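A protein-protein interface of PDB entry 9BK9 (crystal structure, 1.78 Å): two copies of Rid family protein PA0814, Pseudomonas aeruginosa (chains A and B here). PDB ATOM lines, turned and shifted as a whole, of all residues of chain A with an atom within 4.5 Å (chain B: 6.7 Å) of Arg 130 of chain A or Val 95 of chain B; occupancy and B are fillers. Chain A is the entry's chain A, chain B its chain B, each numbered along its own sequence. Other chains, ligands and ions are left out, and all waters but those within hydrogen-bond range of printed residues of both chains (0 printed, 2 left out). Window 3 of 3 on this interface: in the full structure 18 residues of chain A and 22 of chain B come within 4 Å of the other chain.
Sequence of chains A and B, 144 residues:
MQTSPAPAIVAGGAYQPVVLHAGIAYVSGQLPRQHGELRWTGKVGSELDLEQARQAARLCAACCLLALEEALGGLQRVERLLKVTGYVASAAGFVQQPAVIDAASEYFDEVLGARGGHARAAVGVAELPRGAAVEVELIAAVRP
The backbone nitrogen (N) of Pro 129 of chain A sits close to the side-chain amide oxygen (OE1) of Gln 97 of chain B (3.4 Å).
O of Val 95 of chain B lies within hydrogen-bond range of N of Arg 130 of chain A (3.0 Å).
The side-chain carboxylate (OE1) of Glu 127 of chain A sits at hydrogen-bond distance from the backbone NH (N) of Gly 93 of chain B.
The backbone carbonyl oxygen (O) of Phe 94 of chain B sits at hydrogen-bond distance from the side-chain amide nitrogen (NE2) of Gln 97 of chain B (3.0 Å).
The side-chain amide nitrogen of Gln 97 of chain B is in hydrogen-bond range of the side-chain hydroxyl of Ser 90 of chain B, 2.9 Å away.
CB of Ser 90 of chain B touches CG of Glu 127 of chain A, at 3.9 Å.
Ala 92 of chain B touches Glu 127 of chain A.
Glu 127 of chain A touches Phe 94 of chain B (CB to O, 3.3 Å).
Val 95 of chain B touches Glu 127 of chain A.
Glu 127 of chain A touches Gln 97 of chain B.
Leu 128 of chain A touches Val 95 of chain B.
Leu 128 of chain A touches Gln 97 of chain B (C to OE1, 3.5 Å).
Val 95 of chain B touches Pro 129 of chain A (O to CA, 3.7 Å).
Pro 129 of chain A touches Pro 98 of chain B.
CG1 of Val 95 of chain B touches N of Gly 131 of chain A (3.4 Å).
Arg 130 of chain A touches one residue of chain B.
Printed residues of chain A within 4 Å of Val 95 of chain B: Glu 127 (3.9 Å), Leu 128 (3.7 Å), Pro 129 (3.7 Å), Arg 130 (3.0 Å) and Gly 131 (3.4 Å).
Of the printed residues of chain B, Pro 129 of chain A touches Val 95 (3.7 Å), Gln 97 (3.4 Å) and Pro 98 (3.5 Å).
Printed residues of chain B within 4 Å of Glu 127 of chain A: Ser 90 (3.9 Å), Ala 91 (3.7 Å), Ala 92 (3.5 Å), Gly 93 (3.0 Å), Phe 94 (3.3 Å), Val 95 (3.9 Å) and Gln 97 (3.5 Å).
Of the printed residues of chain A, Ala 91 of chain B touches Glu 127 (3.7 Å).
Gln 96 of chain B touches none of the printed residues of chain A.
Ala 99 of chain B touches none of the printed residues of chain A.
Hydrophobic or aromatic side chains of chain A within 4 Å of the printed part of chain B: Pro 129.
Of the 10 printed residues of chain B, 8 touch a printed residue of chain A.
Hydrophobic or aromatic side chains of chain B within 4 Å of the printed part of chain A: Val 95 and Pro 98.
Among the printed residues, no Asp or Glu carboxylate lies within 4 Å of a Lys or Arg side-chain nitrogen of the other chain.
No position is printed for both chains.
Of the 14 pairs that touch across the chains among the printed residues, none has its exchanged pair printed and touching as well.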
ATOM      1  N   ARG A  33       6.364 -18.974 -32.160  1.00  0.00           N
ATOM      2  CA  ARG A  33       6.794 -18.509 -33.475  1.00  0.00           C
ATOM      3  C   ARG A  33       7.945 -19.365 -33.981  1.00  0.00           C
ATOM      4  O   ARG A  33       8.861 -19.697 -33.229  1.00  0.00           O
ATOM      5  CB  ARG A  33       7.234 -17.037 -33.440  1.00  0.00           C
ATOM      6  CG  ARG A  33       6.097 -16.033 -33.332  1.00  0.00           C
ATOM      7  CD  ARG A  33       6.629 -14.598 -33.302  1.00  0.00           C
ATOM      8  NE  ARG A  33       5.629 -13.625 -32.870  1.00  0.00           N
ATOM      9  CZ  ARG A  33       4.810 -13.004 -33.710  1.00  0.00           C
ATOM     10  NH1 ARG A  33       4.864 -13.226 -35.016  1.00  0.00           N
ATOM     11  NH2 ARG A  33       3.934 -12.122 -33.233  1.00  0.00           N
ATOM     12  N   LEU A  38       3.823 -16.670 -36.513  1.00  0.00           N
ATOM     13  CA  LEU A  38       3.018 -17.304 -35.472  1.00  0.00           C
ATOM     14  C   LEU A  38       2.434 -18.610 -36.003  1.00  0.00           C
ATOM     15  O   LEU A  38       1.623 -18.607 -36.934  1.00  0.00           O
ATOM     16  CB  LEU A  38       1.915 -16.357 -35.007  1.00  0.00           C
ATOM     17  CG  LEU A  38       1.226 -16.752 -33.702  1.00  0.00           C
ATOM     18  CD1 LEU A  38       2.206 -16.761 -32.560  1.00  0.00           C
ATOM     19  CD2 LEU A  38       0.111 -15.780 -33.419  1.00  0.00           C
ATOM     20  N   THR A  41      -2.151 -21.148 -33.387  1.00  0.00           N
ATOM     21  CA  THR A  41      -3.191 -20.283 -32.857  1.00  0.00           C
ATOM     22  C   THR A  41      -4.439 -21.114 -32.635  1.00  0.00           C
ATOM     23  O   THR A  41      -4.671 -22.110 -33.323  1.00  0.00           O
ATOM     24  CB  THR A  41      -3.497 -19.096 -33.797  1.00  0.00           C
ATOM     25  OG1 THR A  41      -3.910 -19.584 -35.081  1.00  0.00           O
ATOM     26  CG2 THR A  41      -2.280 -18.210 -33.959  1.00  0.00           C
ATOM     27  N   GLU A 127      -7.442 -16.222 -23.154  1.00  0.00           N
ATOM     28  CA  GLU A 127      -7.000 -15.757 -24.463  1.00  0.00           C
ATOM     29  C   GLU A 127      -5.526 -15.406 -24.386  1.00  0.00           C
ATOM     30  O   GLU A 127      -5.022 -15.041 -23.321  1.00  0.00           O
ATOM     31  CB  GLU A 127      -7.761 -14.495 -24.914  1.00  0.00           C
ATOM     32  CG  GLU A 127      -9.275 -14.592 -25.018  1.00  0.00           C
ATOM     33  CD  GLU A 127      -9.725 -15.471 -26.171  1.00  0.00           C
ATOM     34  OE1 GLU A 127     -10.878 -15.961 -26.127  1.00  0.00           O
ATOM     35  OE2 GLU A 127      -8.950 -15.622 -27.145  1.00  0.00           O
ATOM     36  N   LEU A 128      -4.842 -15.474 -25.523  1.00  0.00           N
ATOM     37  CA  LEU A 128      -3.459 -15.034 -25.582  1.00  0.00           C
ATOM     38  C   LEU A 128      -3.240 -14.089 -26.756  1.00  0.00           C
ATOM     39  O   LEU A 128      -4.057 -14.035 -27.684  1.00  0.00           O
ATOM     40  CB  LEU A 128      -2.497 -16.232 -25.670  1.00  0.00           C
ATOM     41  CG  LEU A 128      -2.315 -17.019 -24.356  1.00  0.00           C
ATOM     42  CD1 LEU A 128      -1.429 -18.238 -24.652  1.00  0.00           C
ATOM     43  CD2 LEU A 128      -1.719 -16.185 -23.207  1.00  0.00           C
ATOM     44  N   PRO A 129      -2.165 -13.295 -26.715  1.00  0.00           N
ATOM     45  CA  PRO A 129      -1.869 -12.361 -27.814  1.00  0.00           C
ATOM     46  C   PRO A 129      -1.926 -13.025 -29.180  1.00  0.00           C
ATOM     47  O   PRO A 129      -1.353 -14.098 -29.393  1.00  0.00           O
ATOM     48  CB  PRO A 129      -0.451 -11.887 -27.485  1.00  0.00           C
ATOM     49  CG  PRO A 129      -0.398 -11.923 -26.006  1.00  0.00           C
ATOM     50  CD  PRO A 129      -1.214 -13.127 -25.601  1.00  0.00           C
ATOM     51  N   ARG A 130      -2.618 -12.370 -30.117  1.00  0.00           N
ATOM     52  CA  ARG A 130      -2.730 -12.811 -31.508  1.00  0.00           C
ATOM     53  C   ARG A 130      -3.407 -14.175 -31.645  1.00  0.00           C
ATOM     54  O   ARG A 130      -3.348 -14.798 -32.717  1.00  0.00           O
ATOM     55  CB  ARG A 130      -1.343 -12.847 -32.174  1.00  0.00           C
ATOM     56  CG  ARG A 130      -0.574 -11.531 -32.128  1.00  0.00           C
ATOM     57  CD  ARG A 130      -0.793 -10.708 -33.383  1.00  0.00           C
ATOM     58  NE  ARG A 130      -0.192 -11.334 -34.556  1.00  0.00           N
ATOM     59  CZ  ARG A 130       0.982 -10.990 -35.073  1.00  0.00           C
ATOM     60  NH1 ARG A 130       1.721 -10.035 -34.535  1.00  0.00           N
ATOM     61  NH2 ARG A 130       1.431 -11.633 -36.150  1.00  0.00           N
ATOM     62  N   GLY A 131      -4.114 -14.637 -30.613  1.00  0.00           N
ATOM     63  CA  GLY A 131      -4.718 -15.952 -30.655  1.00  0.00           C
ATOM     64  C   GLY A 131      -3.750 -17.098 -30.455  1.00  0.00           C
ATOM     65  O   GLY A 131      -4.107 -18.246 -30.747  1.00  0.00           O
ATOM     66  N   ALA A 132      -2.537 -16.822 -29.967  1.00  0.00           N
ATOM     67  CA  ALA A 132      -1.555 -17.867 -29.700  1.00  0.00           C
ATOM     68  C   ALA A 132      -2.110 -18.940 -28.760  1.00  0.00           C
ATOM     69  O   ALA A 132      -2.947 -18.676 -27.886  1.00  0.00           O
ATOM     70  CB  ALA A 132      -0.295 -17.251 -29.087  1.00  0.00           C
ATOM     71  N   SER B  90     -10.572 -10.733 -20.653  1.00  0.00           N
ATOM     72  CA  SER B  90     -10.711 -10.785 -22.102  1.00  0.00           C
ATOM     73  C   SER B  90     -12.002 -11.495 -22.488  1.00  0.00           C
ATOM     74  O   SER B  90     -12.244 -12.629 -22.067  1.00  0.00           O
ATOM     75  CB  SER B  90      -9.503 -11.500 -22.726  1.00  0.00           C
ATOM     76  OG  SER B  90      -8.306 -10.774 -22.499  1.00  0.00           O
ATOM     77  N   ALA B  91     -12.819 -10.840 -23.311  1.00  0.00           N
ATOM     78  CA  ALA B  91     -13.957 -11.548 -23.870  1.00  0.00           C
ATOM     79  C   ALA B  91     -13.488 -12.578 -24.901  1.00  0.00           C
ATOM     80  O   ALA B  91     -12.360 -12.533 -25.398  1.00  0.00           O
ATOM     81  CB  ALA B  91     -14.925 -10.570 -24.534  1.00  0.00           C
ATOM     82  N   ALA B  92     -14.385 -13.503 -25.231  1.00  0.00           N
ATOM     83  CA  ALA B  92     -14.100 -14.511 -26.243  1.00  0.00           C
ATOM     84  C   ALA B  92     -13.638 -13.857 -27.539  1.00  0.00           C
ATOM     85  O   ALA B  92     -14.291 -12.952 -28.061  1.00  0.00           O
ATOM     86  CB  ALA B  92     -15.355 -15.355 -26.490  1.00  0.00           C
ATOM     87  N   GLY B  93     -12.482 -14.292 -28.033  1.00  0.00           N
ATOM     88  CA  GLY B  93     -11.948 -13.795 -29.277  1.00  0.00           C
ATOM     89  C   GLY B  93     -11.113 -12.536 -29.180  1.00  0.00           C
ATOM     90  O   GLY B  93     -10.567 -12.095 -30.201  1.00  0.00           O
ATOM     91  N   PHE B  94     -11.015 -11.912 -28.004  1.00  0.00           N
ATOM     92  CA  PHE B  94     -10.190 -10.720 -27.878  1.00  0.00           C
ATOM     93  C   PHE B  94      -8.733 -11.146 -27.759  1.00  0.00           C
ATOM     94  O   PHE B  94      -8.379 -11.902 -26.846  1.00  0.00           O
ATOM     95  CB  PHE B  94     -10.592  -9.861 -26.679  1.00  0.00           C
ATOM     96  CG  PHE B  94      -9.724  -8.665 -26.527  1.00  0.00           C
ATOM     97  CD1 PHE B  94      -9.890  -7.575 -27.367  1.00  0.00           C
ATOM     98  CD2 PHE B  94      -8.689  -8.653 -25.609  1.00  0.00           C
ATOM     99  CE1 PHE B  94      -9.062  -6.482 -27.279  1.00  0.00           C
ATOM    100  CE2 PHE B  94      -7.857  -7.552 -25.506  1.00  0.00           C
ATOM    101  CZ  PHE B  94      -8.039  -6.466 -26.332  1.00  0.00           C
ATOM    102  N   VAL B  95      -7.892 -10.676 -28.680  1.00  0.00           N
ATOM    103  CA  VAL B  95      -6.505 -11.129 -28.739  1.00  0.00           C
ATOM    104  C   VAL B  95      -5.538  -9.954 -28.837  1.00  0.00           C
ATOM    105  O   VAL B  95      -4.393 -10.114 -29.266  1.00  0.00           O
ATOM    106  CB  VAL B  95      -6.303 -12.103 -29.920  1.00  0.00           C
ATOM    107  CG1 VAL B  95      -7.100 -13.379 -29.703  1.00  0.00           C
ATOM    108  CG2 VAL B  95      -6.743 -11.452 -31.237  1.00  0.00           C
ATOM    109  N   GLN B  96      -5.956  -8.769 -28.401  1.00  0.00           N
ATOM    110  CA  GLN B  96      -5.084  -7.600 -28.469  1.00  0.00           C
ATOM    111  C   GLN B  96      -4.557  -7.187 -27.097  1.00  0.00           C
ATOM    112  O   GLN B  96      -4.388  -5.999 -26.823  1.00  0.00           O
ATOM    113  CB  GLN B  96      -5.821  -6.446 -29.135  1.00  0.00           C
ATOM    114  CG  GLN B  96      -6.229  -6.798 -30.560  1.00  0.00           C
ATOM    115  CD  GLN B  96      -7.206  -5.808 -31.160  1.00  0.00           C
ATOM    116  OE1 GLN B  96      -6.812  -4.755 -31.659  1.00  0.00           O
ATOM    117  NE2 GLN B  96      -8.493  -6.148 -31.118  1.00  0.00           N
ATOM    118  N   GLN B  97      -4.277  -8.162 -26.225  1.00  0.00           N
ATOM    119  CA  GLN B  97      -3.680  -7.840 -24.928  1.00  0.00           C
ATOM    120  C   GLN B  97      -2.368  -7.063 -25.022  1.00  0.00           C
ATOM    121  O   GLN B  97      -2.140  -6.202 -24.149  1.00  0.00           O
ATOM    122  CB  GLN B  97      -3.461  -9.120 -24.103  1.00  0.00           C
ATOM    123  CG  GLN B  97      -4.723  -9.868 -23.724  1.00  0.00           C
ATOM    124  CD  GLN B  97      -5.224 -10.753 -24.852  1.00  0.00           C
ATOM    125  OE1 GLN B  97      -4.525 -10.955 -25.853  1.00  0.00           O
ATOM    126  NE2 GLN B  97      -6.443 -11.285 -24.703  1.00  0.00           N
ATOM    127  N   PRO B  98      -1.453  -7.325 -25.983  1.00  0.00           N
ATOM    128  CA  PRO B  98      -0.241  -6.491 -26.047  1.00  0.00           C
ATOM    129  C   PRO B  98      -0.552  -5.026 -26.244  1.00  0.00           C
ATOM    130  O   PRO B  98       0.103  -4.184 -25.630  1.00  0.00           O
ATOM    131  CB  PRO B  98       0.532  -7.070 -27.238  1.00  0.00           C
ATOM    132  CG  PRO B  98       0.081  -8.477 -27.320  1.00  0.00           C
ATOM    133  CD  PRO B  98      -1.382  -8.436 -26.952  1.00  0.00           C
ATOM    134  N   ALA B  99      -1.533  -4.694 -27.087  1.00  0.00           N
ATOM    135  CA  ALA B  99      -1.894  -3.293 -27.277  1.00  0.00           C
ATOM    136  C   ALA B  99      -2.448  -2.670 -25.999  1.00  0.00           C
ATOM    137  O   ALA B  99      -2.241  -1.473 -25.752  1.00  0.00           O
ATOM    138  CB  ALA B  99      -2.926  -3.166 -28.394  1.00  0.00           C
